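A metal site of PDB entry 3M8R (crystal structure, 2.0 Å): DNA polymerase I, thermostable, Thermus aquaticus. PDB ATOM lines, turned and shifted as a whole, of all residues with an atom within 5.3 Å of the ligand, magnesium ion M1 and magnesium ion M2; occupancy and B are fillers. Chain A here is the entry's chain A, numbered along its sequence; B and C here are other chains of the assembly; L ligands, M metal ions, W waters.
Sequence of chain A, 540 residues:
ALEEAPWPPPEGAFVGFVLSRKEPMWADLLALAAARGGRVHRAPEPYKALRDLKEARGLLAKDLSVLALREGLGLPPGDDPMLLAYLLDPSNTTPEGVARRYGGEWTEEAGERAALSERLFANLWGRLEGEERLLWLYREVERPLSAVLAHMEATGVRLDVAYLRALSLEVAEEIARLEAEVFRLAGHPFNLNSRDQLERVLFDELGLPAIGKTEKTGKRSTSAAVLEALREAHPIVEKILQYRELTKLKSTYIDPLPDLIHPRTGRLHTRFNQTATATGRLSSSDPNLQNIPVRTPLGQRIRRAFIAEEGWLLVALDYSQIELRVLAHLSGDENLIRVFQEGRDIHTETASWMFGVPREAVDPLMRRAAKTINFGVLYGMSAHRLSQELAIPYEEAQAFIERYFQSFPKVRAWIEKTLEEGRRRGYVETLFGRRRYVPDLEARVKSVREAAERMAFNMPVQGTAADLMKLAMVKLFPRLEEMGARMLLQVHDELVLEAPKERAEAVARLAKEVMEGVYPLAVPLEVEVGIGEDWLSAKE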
ATOM      1  N   ARG A 281       1.335  11.989  27.888  1.00  0.00           N
ATOM      2  CA  ARG A 281       2.106  10.815  27.501  1.00  0.00           C
ATOM      3  C   ARG A 281       2.697  10.140  28.732  1.00  0.00           C
ATOM      4  O   ARG A 281       2.915  10.786  29.762  1.00  0.00           O
ATOM      5  CB  ARG A 281       3.260  11.207  26.583  1.00  0.00           C
ATOM      6  CG  ARG A 281       2.904  11.356  25.130  1.00  0.00           C
ATOM      7  CD  ARG A 281       4.169  11.408  24.291  1.00  0.00           C
ATOM      8  NE  ARG A 281       3.896  11.553  22.867  1.00  0.00           N
ATOM      9  CZ  ARG A 281       4.840  11.530  21.933  1.00  0.00           C
ATOM     10  NH1 ARG A 281       6.110  11.368  22.276  1.00  0.00           N
ATOM     11  NH2 ARG A 281       4.517  11.665  20.648  1.00  0.00           N
ATOM     12  N   ASP A 318       1.171  -0.887  16.240  1.00  0.00           N
ATOM     13  CA  ASP A 318       1.523   0.521  16.148  1.00  0.00           C
ATOM     14  C   ASP A 318       0.453   1.277  15.355  1.00  0.00           C
ATOM     15  O   ASP A 318       0.153   0.930  14.223  1.00  0.00           O
ATOM     16  CB  ASP A 318       2.876   0.655  15.449  1.00  0.00           C
ATOM     17  CG  ASP A 318       3.417   2.081  15.456  1.00  0.00           C
ATOM     18  OD1 ASP A 318       2.657   3.008  15.111  1.00  0.00           O
ATOM     19  OD2 ASP A 318       4.595   2.276  15.804  1.00  0.00           O
ATOM     20  N   TYR A 319      -0.118   2.312  15.965  1.00  0.00           N
ATOM     21  CA  TYR A 319      -1.135   3.112  15.288  1.00  0.00           C
ATOM     22  C   TYR A 319      -0.551   3.782  14.070  1.00  0.00           C
ATOM     23  O   TYR A 319       0.556   4.314  14.109  1.00  0.00           O
ATOM     24  CB  TYR A 319      -1.696   4.194  16.215  1.00  0.00           C
ATOM     25  CG  TYR A 319      -2.741   3.728  17.212  1.00  0.00           C
ATOM     26  CD1 TYR A 319      -4.032   3.427  16.805  1.00  0.00           C
ATOM     27  CD2 TYR A 319      -2.434   3.626  18.561  1.00  0.00           C
ATOM     28  CE1 TYR A 319      -4.989   3.024  17.723  1.00  0.00           C
ATOM     29  CE2 TYR A 319      -3.374   3.222  19.478  1.00  0.00           C
ATOM     30  CZ  TYR A 319      -4.649   2.918  19.055  1.00  0.00           C
ATOM     31  OH  TYR A 319      -5.587   2.526  19.979  1.00  0.00           O
ATOM     32  N   SER A 320      -1.304   3.776  12.977  1.00  0.00           N
ATOM     33  CA  SER A 320      -0.889   4.404  11.731  1.00  0.00           C
ATOM     34  C   SER A 320      -1.102   5.928  11.790  1.00  0.00           C
ATOM     35  O   SER A 320      -2.177   6.395  12.155  1.00  0.00           O
ATOM     36  CB  SER A 320      -1.675   3.811  10.564  1.00  0.00           C
ATOM     37  OG  SER A 320      -1.389   4.473   9.347  1.00  0.00           O
ATOM     38  N   GLN A 321      -0.049   6.669  11.438  1.00  0.00           N
ATOM     39  CA  GLN A 321      -0.127   8.124  11.290  1.00  0.00           C
ATOM     40  C   GLN A 321      -1.030   8.783  12.325  1.00  0.00           C
ATOM     41  O   GLN A 321      -1.855   9.633  11.987  1.00  0.00           O
ATOM     42  CB  GLN A 321      -0.651   8.475   9.894  1.00  0.00           C
ATOM     43  CG  GLN A 321      -0.138   7.564   8.795  1.00  0.00           C
ATOM     44  CD  GLN A 321      -0.804   7.845   7.461  1.00  0.00           C
ATOM     45  OE1 GLN A 321      -0.535   8.864   6.818  1.00  0.00           O
ATOM     46  NE2 GLN A 321      -1.684   6.949   7.032  1.00  0.00           N
ATOM     47  N   ILE A 322      -0.866   8.412  13.592  1.00  0.00           N
ATOM     48  CA  ILE A 322      -1.943   8.658  14.552  1.00  0.00           C
ATOM     49  C   ILE A 322      -2.180  10.114  14.941  1.00  0.00           C
ATOM     50  O   ILE A 322      -3.331  10.542  15.021  1.00  0.00           O
ATOM     51  CB  ILE A 322      -1.802   7.794  15.841  1.00  0.00           C
ATOM     52  CG1 ILE A 322      -3.166   7.680  16.519  1.00  0.00           C
ATOM     53  CG2 ILE A 322      -0.738   8.377  16.762  1.00  0.00           C
ATOM     54  CD1 ILE A 322      -3.129   7.292  17.988  1.00  0.00           C
ATOM     55  N   GLU A 323      -1.140  10.904  15.148  1.00  0.00           N
ATOM     56  CA  GLU A 323      -1.375  12.300  15.497  1.00  0.00           C
ATOM     57  C   GLU A 323      -2.001  13.051  14.331  1.00  0.00           C
ATOM     58  O   GLU A 323      -2.749  14.002  14.523  1.00  0.00           O
ATOM     59  CB  GLU A 323      -0.111  12.983  16.059  1.00  0.00           C
ATOM     60  CG  GLU A 323       0.041  12.725  17.573  1.00  0.00           C
ATOM     61  CD  GLU A 323       1.338  13.249  18.165  1.00  0.00           C
ATOM     62  OE1 GLU A 323       1.845  14.306  17.709  1.00  0.00           O
ATOM     63  OE2 GLU A 323       1.844  12.622  19.116  1.00  0.00           O
ATOM     64  N   LEU A 324      -1.731  12.601  13.096  1.00  0.00           N
ATOM     65  CA  LEU A 324      -2.360  13.208  11.927  1.00  0.00           C
ATOM     66  C   LEU A 324      -3.854  12.919  11.910  1.00  0.00           C
ATOM     67  O   LEU A 324      -4.660  13.792  11.570  1.00  0.00           O
ATOM     68  CB  LEU A 324      -1.700  12.748  10.629  1.00  0.00           C
ATOM     69  CG  LEU A 324      -0.247  13.197  10.403  1.00  0.00           C
ATOM     70  CD1 LEU A 324       0.291  12.642   9.088  1.00  0.00           C
ATOM     71  CD2 LEU A 324      -0.144  14.711  10.433  1.00  0.00           C
ATOM     72  N   HIS A 347       2.955   9.990   4.949  1.00  0.00           N
ATOM     73  CA  HIS A 347       4.374   9.757   5.191  1.00  0.00           C
ATOM     74  C   HIS A 347       5.056   9.190   3.950  1.00  0.00           C
ATOM     75  O   HIS A 347       6.197   9.531   3.659  1.00  0.00           O
ATOM     76  CB  HIS A 347       4.563   8.803   6.380  1.00  0.00           C
ATOM     77  CG  HIS A 347       4.077   9.365   7.685  1.00  0.00           C
ATOM     78  ND1 HIS A 347       4.000  10.723   7.930  1.00  0.00           N
ATOM     79  CD2 HIS A 347       3.643   8.756   8.811  1.00  0.00           C
ATOM     80  CE1 HIS A 347       3.542  10.923   9.150  1.00  0.00           C
ATOM     81  NE2 HIS A 347       3.321   9.748   9.709  1.00  0.00           N
ATOM     82  N   ARG A 367      10.899   6.360   4.540  1.00  0.00           N
ATOM     83  CA  ARG A 367       9.623   6.744   5.127  1.00  0.00           C
ATOM     84  C   ARG A 367       9.793   7.358   6.517  1.00  0.00           C
ATOM     85  O   ARG A 367       9.116   8.317   6.874  1.00  0.00           O
ATOM     86  CB  ARG A 367       8.698   5.538   5.214  1.00  0.00           C
ATOM     87  CG  ARG A 367       7.289   5.875   5.635  1.00  0.00           C
ATOM     88  CD  ARG A 367       6.345   4.710   5.409  1.00  0.00           C
ATOM     89  NE  ARG A 367       4.983   5.035   5.841  1.00  0.00           N
ATOM     90  CZ  ARG A 367       4.580   4.993   7.106  1.00  0.00           C
ATOM     91  NH1 ARG A 367       5.428   4.642   8.061  1.00  0.00           N
ATOM     92  NH2 ARG A 367       3.331   5.316   7.424  1.00  0.00           N
ATOM     93  N   LYS A 371       8.823  11.127   7.976  1.00  0.00           N
ATOM     94  CA  LYS A 371       8.000  11.373   9.157  1.00  0.00           C
ATOM     95  C   LYS A 371       8.494  12.568   9.968  1.00  0.00           C
ATOM     96  O   LYS A 371       7.692  13.378  10.424  1.00  0.00           O
ATOM     97  CB  LYS A 371       7.923  10.118  10.041  1.00  0.00           C
ATOM     98  CG  LYS A 371       6.958   9.076   9.516  1.00  0.00           C
ATOM     99  CD  LYS A 371       6.643   8.013  10.554  1.00  0.00           C
ATOM    100  CE  LYS A 371       7.682   6.909  10.571  1.00  0.00           C
ATOM    101  NZ  LYS A 371       7.394   5.888  11.599  1.00  0.00           N
ATOM    102  N   THR A 372       9.803  12.687  10.138  1.00  0.00           N
ATOM    103  CA  THR A 372      10.355  13.801  10.890  1.00  0.00           C
ATOM    104  C   THR A 372      10.052  15.106  10.161  1.00  0.00           C
ATOM    105  O   THR A 372       9.937  16.159  10.772  1.00  0.00           O
ATOM    106  CB  THR A 372      11.884  13.684  11.128  1.00  0.00           C
ATOM    107  OG1 THR A 372      12.579  14.450  10.127  1.00  0.00           O
ATOM    108  CG2 THR A 372      12.355  12.230  11.083  1.00  0.00           C
ATOM    109  N   PHE A 375       5.888  15.864  10.674  1.00  0.00           N
ATOM    110  CA  PHE A 375       5.561  16.383  11.989  1.00  0.00           C
ATOM    111  C   PHE A 375       6.375  17.642  12.299  1.00  0.00           C
ATOM    112  O   PHE A 375       5.926  18.518  13.039  1.00  0.00           O
ATOM    113  CB  PHE A 375       5.789  15.319  13.058  1.00  0.00           C
ATOM    114  CG  PHE A 375       4.863  14.147  12.931  1.00  0.00           C
ATOM    115  CD1 PHE A 375       3.493  14.307  13.070  1.00  0.00           C
ATOM    116  CD2 PHE A 375       5.360  12.888  12.651  1.00  0.00           C
ATOM    117  CE1 PHE A 375       2.635  13.235  12.949  1.00  0.00           C
ATOM    118  CE2 PHE A 375       4.507  11.800  12.531  1.00  0.00           C
ATOM    119  CZ  PHE A 375       3.145  11.979  12.676  1.00  0.00           C
ATOM    120  N   TYR A 379       4.228  21.091  13.357  1.00  0.00           N
ATOM    121  CA  TYR A 379       4.349  21.739  14.664  1.00  0.00           C
ATOM    122  C   TYR A 379       5.243  22.979  14.657  1.00  0.00           C
ATOM    123  O   TYR A 379       5.704  23.419  15.710  1.00  0.00           O
ATOM    124  CB  TYR A 379       4.814  20.734  15.714  1.00  0.00           C
ATOM    125  CG  TYR A 379       3.803  19.627  15.939  1.00  0.00           C
ATOM    126  CD1 TYR A 379       2.481  19.931  16.233  1.00  0.00           C
ATOM    127  CD2 TYR A 379       4.167  18.289  15.856  1.00  0.00           C
ATOM    128  CE1 TYR A 379       1.550  18.939  16.435  1.00  0.00           C
ATOM    129  CE2 TYR A 379       3.234  17.285  16.065  1.00  0.00           C
ATOM    130  CZ  TYR A 379       1.933  17.624  16.350  1.00  0.00           C
ATOM    131  OH  TYR A 379       0.986  16.646  16.560  1.00  0.00           O
ATOM    132  N   ALA A 465      -3.762  11.704  21.434  1.00  0.00           N
ATOM    133  CA  ALA A 465      -3.185  10.428  21.000  1.00  0.00           C
ATOM    134  C   ALA A 465      -2.779   9.594  22.213  1.00  0.00           C
ATOM    135  O   ALA A 465      -2.977   8.390  22.231  1.00  0.00           O
ATOM    136  CB  ALA A 465      -1.999  10.674  20.076  1.00  0.00           C
ATOM    137  N   VAL A 491       5.188   2.231  23.726  1.00  0.00           N
ATOM    138  CA  VAL A 491       6.063   3.266  23.173  1.00  0.00           C
ATOM    139  C   VAL A 491       5.196   4.305  22.464  1.00  0.00           C
ATOM    140  O   VAL A 491       5.213   4.418  21.240  1.00  0.00           O
ATOM    141  CB  VAL A 491       7.100   2.682  22.190  1.00  0.00           C
ATOM    142  CG1 VAL A 491       8.137   3.741  21.823  1.00  0.00           C
ATOM    143  CG2 VAL A 491       7.792   1.468  22.803  1.00  0.00           C
ATOM    144  N   HIS A 492       4.428   5.025  23.274  1.00  0.00           N
ATOM    145  CA  HIS A 492       3.590   6.157  22.851  1.00  0.00           C
ATOM    146  C   HIS A 492       2.363   5.761  22.016  1.00  0.00           C
ATOM    147  O   HIS A 492       1.237   5.925  22.477  1.00  0.00           O
ATOM    148  CB  HIS A 492       4.454   7.218  22.177  1.00  0.00           C
ATOM    149  CG  HIS A 492       5.657   7.578  22.994  1.00  0.00           C
ATOM    150  ND1 HIS A 492       5.570   7.996  24.301  1.00  0.00           N
ATOM    151  CD2 HIS A 492       6.976   7.529  22.707  1.00  0.00           C
ATOM    152  CE1 HIS A 492       6.777   8.217  24.774  1.00  0.00           C
ATOM    153  NE2 HIS A 492       7.655   7.946  23.837  1.00  0.00           N
ATOM    154  N   ASP A 493       2.559   5.258  20.795  1.00  0.00           N
ATOM    155  CA  ASP A 493       1.431   4.756  20.012  1.00  0.00           C
ATOM    156  C   ASP A 493       1.662   3.305  19.602  1.00  0.00           C
ATOM    157  O   ASP A 493       1.041   2.814  18.654  1.00  0.00           O
ATOM    158  CB  ASP A 493       1.189   5.619  18.780  1.00  0.00           C
ATOM    159  CG  ASP A 493       2.163   5.329  17.659  1.00  0.00           C
ATOM    160  OD1 ASP A 493       3.339   5.047  17.977  1.00  0.00           O
ATOM    161  OD2 ASP A 493       1.761   5.397  16.488  1.00  0.00           O
ATOM    162  N   GLU A 494       2.542   2.626  20.328  1.00  0.00           N
ATOM    163  CA  GLU A 494       2.880   1.238  20.029  1.00  0.00           C
ATOM    164  C   GLU A 494       2.748   0.395  21.289  1.00  0.00           C
ATOM    165  O   GLU A 494       3.012   0.875  22.391  1.00  0.00           O
ATOM    166  CB  GLU A 494       4.313   1.162  19.507  1.00  0.00           C
ATOM    167  CG  GLU A 494       4.813  -0.257  19.253  1.00  0.00           C
ATOM    168  CD  GLU A 494       6.259  -0.300  18.786  1.00  0.00           C
ATOM    169  OE1 GLU A 494       6.915   0.774  18.773  1.00  0.00           O
ATOM    170  OE2 GLU A 494       6.757  -1.392  18.453  1.00  0.00           O
ATOM    171  N   LYS A 539       7.926  -6.040  13.698  1.00  0.00           N
ATOM    172  CA  LYS A 539       7.440  -4.852  13.007  1.00  0.00           C
ATOM    173  C   LYS A 539       7.751  -4.924  11.510  1.00  0.00           C
ATOM    174  O   LYS A 539       7.080  -4.301  10.699  1.00  0.00           O
ATOM    175  CB  LYS A 539       8.054  -3.581  13.601  1.00  0.00           C
ATOM    176  CG  LYS A 539       7.743  -3.378  15.079  1.00  0.00           C
ATOM    177  CD  LYS A 539       7.908  -1.923  15.489  1.00  0.00           C
ATOM    178  CE  LYS A 539       6.658  -1.124  15.219  1.00  0.00           C
ATOM    179  NZ  LYS A 539       6.884   0.338  15.404  1.00  0.00           N
ATOM    180  P    DA B   4      12.827  25.324  14.319  1.00  0.00           P
ATOM    181  OP1  DA B   4      14.025  24.603  14.818  1.00  0.00           O
ATOM    182  OP2  DA B   4      12.816  25.856  12.936  1.00  0.00           O
ATOM    183  O5'  DA B   4      11.535  24.402  14.496  1.00  0.00           O
ATOM    184  C5'  DA B   4      11.297  23.741  15.744  1.00  0.00           C
ATOM    185  C4'  DA B   4       9.850  23.262  15.842  1.00  0.00           C
ATOM    186  O4'  DA B   4       9.589  22.319  14.773  1.00  0.00           O
ATOM    187  C3'  DA B   4       9.502  22.527  17.122  1.00  0.00           C
ATOM    188  O3'  DA B   4       9.027  23.470  18.060  1.00  0.00           O
ATOM    189  C2'  DA B   4       8.385  21.584  16.690  1.00  0.00           C
ATOM    190  C1'  DA B   4       8.770  21.269  15.252  1.00  0.00           C
ATOM    191  N9   DA B   4       9.488  20.012  15.049  1.00  0.00           N
ATOM    192  C8   DA B   4      10.766  19.862  14.583  1.00  0.00           C
ATOM    193  N7   DA B   4      11.156  18.620  14.495  1.00  0.00           N
ATOM    194  C5   DA B   4      10.052  17.890  14.930  1.00  0.00           C
ATOM    195  C6   DA B   4       9.828  16.509  15.076  1.00  0.00           C
ATOM    196  N6   DA B   4      10.735  15.584  14.779  1.00  0.00           N
ATOM    197  N1   DA B   4       8.625  16.118  15.537  1.00  0.00           N
ATOM    198  C2   DA B   4       7.714  17.048  15.841  1.00  0.00           C
ATOM    199  N3   DA B   4       7.807  18.374  15.742  1.00  0.00           N
ATOM    200  C4   DA B   4       9.019  18.731  15.281  1.00  0.00           C
ATOM    201  P    DG B   5       9.548  23.476  19.575  1.00  0.00           P
ATOM    202  OP1  DG B   5       9.295  24.816  20.139  1.00  0.00           O
ATOM    203  OP2  DG B   5      10.920  22.919  19.588  1.00  0.00           O
ATOM    204  O5'  DG B   5       8.585  22.427  20.313  1.00  0.00           O
ATOM    205  C5'  DG B   5       7.179  22.709  20.430  1.00  0.00           C
ATOM    206  C4'  DG B   5       6.403  21.429  20.678  1.00  0.00           C
ATOM    207  O4'  DG B   5       6.555  20.535  19.549  1.00  0.00           O
ATOM    208  C3'  DG B   5       6.917  20.603  21.847  1.00  0.00           C
ATOM    209  O3'  DG B   5       6.369  21.090  23.051  1.00  0.00           O
ATOM    210  C2'  DG B   5       6.335  19.224  21.522  1.00  0.00           C
ATOM    211  C1'  DG B   5       6.528  19.199  20.012  1.00  0.00           C
ATOM    212  N9   DG B   5       7.745  18.522  19.579  1.00  0.00           N
ATOM    213  C8   DG B   5       8.922  19.086  19.165  1.00  0.00           C
ATOM    214  N7   DG B   5       9.824  18.201  18.839  1.00  0.00           N
ATOM    215  C5   DG B   5       9.203  16.983  19.053  1.00  0.00           C
ATOM    216  C6   DG B   5       9.703  15.678  18.874  1.00  0.00           C
ATOM    217  O6   DG B   5      10.827  15.336  18.474  1.00  0.00           O
ATOM    218  N1   DG B   5       8.744  14.722  19.211  1.00  0.00           N
ATOM    219  C2   DG B   5       7.472  15.010  19.659  1.00  0.00           C
ATOM    220  N2   DG B   5       6.681  13.971  19.944  1.00  0.00           N
ATOM    221  N3   DG B   5       7.000  16.239  19.838  1.00  0.00           N
ATOM    222  C4   DG B   5       7.928  17.169  19.510  1.00  0.00           C
ATOM    223  N1  DOC C  12       8.762   9.720  18.891  1.00  0.00           N
ATOM    224  C2  DOC C  12       8.487  11.099  19.101  1.00  0.00           C
ATOM    225  N3  DOC C  12       9.407  12.120  18.531  1.00  0.00           N
ATOM    226  C4  DOC C  12      10.510  11.740  17.800  1.00  0.00           C
ATOM    227  C5  DOC C  12      10.809  10.271  17.556  1.00  0.00           C
ATOM    228  C6  DOC C  12       9.962   9.304  18.098  1.00  0.00           C
ATOM    229  O2  DOC C  12       7.506  11.419  19.747  1.00  0.00           O
ATOM    230  N4  DOC C  12      11.383  12.738  17.255  1.00  0.00           N
ATOM    231  C1' DOC C  12       7.868   8.705  19.488  1.00  0.00           C
ATOM    232  C2' DOC C  12       6.629   8.389  18.687  1.00  0.00           C
ATOM    233  C3' DOC C  12       6.956   7.061  18.082  1.00  0.00           C
ATOM    234  C4' DOC C  12       7.900   6.449  19.107  1.00  0.00           C
ATOM    235  O4' DOC C  12       8.511   7.482  19.829  1.00  0.00           O
ATOM    236  C5' DOC C  12       8.843   5.405  18.584  1.00  0.00           C
ATOM    237  O5' DOC C  12       9.581   5.973  17.549  1.00  0.00           O
ATOM    238  P   DOC C  12      10.765   5.173  16.902  1.00  0.00           P
ATOM    239  OP1 DOC C  12      10.308   3.789  16.541  1.00  0.00           O
ATOM    240  OP2 DOC C  12      11.221   5.901  15.686  1.00  0.00           O
HETATM  241  C1  LIG L   1       2.284   9.586  17.932  1.00  0.00           C
HETATM  242  N1  LIG L   1       6.170  11.889  16.179  1.00  0.00           N
HETATM  243  O1  LIG L   1       4.533   7.744  13.398  1.00  0.00           O
HETATM  244  P1  LIG L   1       5.121   7.009  14.665  1.00  0.00           P
HETATM  245  C2  LIG L   1       6.643  13.280  16.178  1.00  0.00           C
HETATM  246  O2  LIG L   1       5.967  14.133  16.701  1.00  0.00           O
HETATM  247  P2  LIG L   1       3.061   7.587  12.858  1.00  0.00           P
HETATM  248  C3  LIG L   1       2.563   9.209  19.347  1.00  0.00           C
HETATM  249  N2  LIG L   1       7.876  13.594  15.582  1.00  0.00           N
HETATM  250  O3  LIG L   1       3.064   6.849  11.459  1.00  0.00           O
HETATM  251  P3  LIG L   1       3.171   5.281  11.359  1.00  0.00           P
HETATM  252  C4  LIG L   1       8.646  12.614  14.999  1.00  0.00           C
HETATM  253  O4  LIG L   1       9.714  12.905  14.487  1.00  0.00           O
HETATM  254  C5  LIG L   1       8.187  11.250  14.991  1.00  0.00           C
HETATM  255  O5  LIG L   1       4.590   4.886  10.832  1.00  0.00           O
HETATM  256  C6  LIG L   1       6.914  10.921  15.612  1.00  0.00           C
HETATM  257  O6  LIG L   1       2.090   4.771  10.353  1.00  0.00           O
HETATM  258  O7  LIG L   1       2.974   4.660  12.716  1.00  0.00           O
HETATM  259  O8  LIG L   1       2.492   9.020  12.634  1.00  0.00           O
HETATM  260  O9  LIG L   1       2.191   6.837  13.843  1.00  0.00           O
HETATM  261  C7  LIG L   1       4.906  11.526  16.814  1.00  0.00           C
HETATM  262  O10 LIG L   1       4.369   5.676  14.991  1.00  0.00           O
HETATM  263  O11 LIG L   1       6.575   6.661  14.404  1.00  0.00           O
HETATM  264  C8  LIG L   1       3.627  11.736  16.037  1.00  0.00           C
HETATM  265  C9  LIG L   1       3.191  10.375  15.702  1.00  0.00           C
HETATM  266  O12 LIG L   1       1.991  10.172  15.044  1.00  0.00           O
HETATM  267  C10 LIG L   1       3.468   9.592  16.987  1.00  0.00           C
HETATM  268  O13 LIG L   1       4.619  10.301  17.649  1.00  0.00           O
HETATM  269  C11 LIG L   1       3.854   8.168  16.607  1.00  0.00           C
HETATM  270  O14 LIG L   1       5.049   7.978  15.921  1.00  0.00           O
HETATM  271  C12 LIG L   1       9.012  10.153  14.357  1.00  0.00           C
HETATM  272 MG    MG M   1       2.639   4.926  14.507  1.00  0.00          MG
HETATM  273 MG    MG M   2       4.993   4.324  16.797  1.00  0.00          MG
HETATM  274  O   HOH W   1       7.300   4.226  15.431  1.00  0.00           O
HETATM  275  O   HOH W   2       6.305   3.405  18.527  1.00  0.00           O
HETATM  276  O   HOH W   3       1.999   2.133  12.041  1.00  0.00           O
HETATM  277  O   HOH W   4       3.865  15.379  18.964  1.00  0.00           O
HETATM  278  O   HOH W   5       5.839   3.408  13.093  1.00  0.00           O
HETATM  279  O   HOH W   6       1.121  11.161  21.663  1.00  0.00           O
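O2 of DOC 12 of chain C lies close to N2 of DG 5 of chain B (2.7 Å).
OE1 of Glu 323 is in hydrogen-bond range of OH of Tyr 379, at 2.7 Å.
OD2 of Asp 318 lies close to NZ of Lys 539.
N2 of DG 5 of chain B is in hydrogen-bond range of the guanidinium group (NH2) of Arg 281, 3.2 Å away.
The guanidinium group of Arg 281 lies within salt-bridge range of the side-chain carboxylate of Glu 323, at 3.2 Å.
O2 of DOC 12 of chain C is in hydrogen-bond range of the guanidinium group of Arg 281 (2.9 Å).
NE2 of Gln 321 sits close to OG of Ser 320 (3.4 Å).
An oxygen (O2) of the ligand lies close to N2 of DG 5 of chain B (3.3 Å).
N4 of DOC 12 of chain C sits close to an oxygen (O4) of the ligand (3.2 Å).
Residues that only touch the ligand: Phe 375 (3.0 Å), Ser 320 (3.3 Å), Thr 372 (3.8 Å) and His 492 (3.9 Å).
Hydrophobic or aromatic side chains that line the ligand: Ile 322, His 347, Phe 375 and His 492.
17 residues have an atom within 4 Å of the ligand: Arg 281, Asp 318, Tyr 319, Ser 320, Gln 321, Ile 322, Glu 323, His 347, Arg 367, Lys 371, Thr 372, Phe 375, His 492, Asp 493, DA 4 of chain B, DG 5 of chain B and DOC 12 of chain C.
The nearest printed residue that does not touch the ligand is Tyr 379 (4.2 Å).
C3' of DOC 12 of chain C touches magnesium ion M2, at 3.6 Å.
Along chain A the residues within 4 Å of magnesium ion M2 span positions 318 to 493.
Water W2 lies within hydrogen-bond range of the side-chain carboxylate of Glu 494 and the backbone carbonyl oxygen of Val 491.
Water W1 bridges an oxygen (O11) of the ligand and OP1 of DOC 12 of chain C.
Water W3 bridges O of Asp 318 (3.1 Å) and O6 of the ligand (3.1 Å).
Water W5 lies within hydrogen-bond range of an oxygen (O5) of the ligand (3.0 Å) and the side-chain amino group of Lys 371 (3.3 Å).
Water W6 lies within hydrogen-bond range of the side-chain carboxylate (OE2) of Glu 323 (3.0 Å) and the guanidinium group (NE) of Arg 281 (3.1 Å).
Three residues have an atom within 4 Å of magnesium ion M1: Asp 318, Tyr 319 and Asp 493.
Magnesium ion M2 is bound by OD1 of Asp 493.
OD2 of Asp 318 binds magnesium ion M2 (2.3 Å).
An oxygen (O10) of the ligand is bound to magnesium ion M2 (2.3 Å).
Water W2 binds magnesium ion M2 (2.4 Å).
Slightly farther from magnesium ion M2 lies water W1 (2.7 Å).
Magnesium ion M1 is bound by O7 of the ligand (1.8 Å), O10 of the ligand (1.9 Å), OD1 of Asp 318 (2.0 Å), O9 of the ligand (2.1 Å), O of Tyr 319 (2.2 Å) and OD2 of Asp 493 (2.2 Å).
Magnesium ion M1 has six donor atoms within binding distance.
An oxygen (O11) of the ligand is in salt-bridge range of the side-chain amino group (NZ) of Lys 371, 3.0 Å away.
The backbone NH (N) of Gln 321 sits at hydrogen-bond distance from an oxygen (O6) of the ligand (3.1 Å).
A ring nitrogen (NE2) of His 347 lies within hydrogen-bond range of an oxygen (O8) of the ligand, at 3.1 Å.
N of Ile 322 sits close to O9 of the ligand.
An oxygen (O12) of the ligand sits at hydrogen-bond distance from the backbone NH (N) of Glu 323 (3.2 Å).
O5 of the ligand lies within salt-bridge range of NH1 of Arg 367 (2.9 Å).
N2 of the ligand lies within hydrogen-bond range of N1 of DA 4 of chain B (2.6 Å).
NH2 of Arg 281 lies within hydrogen-bond range of O13 of the ligand, at 3.3 Å.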
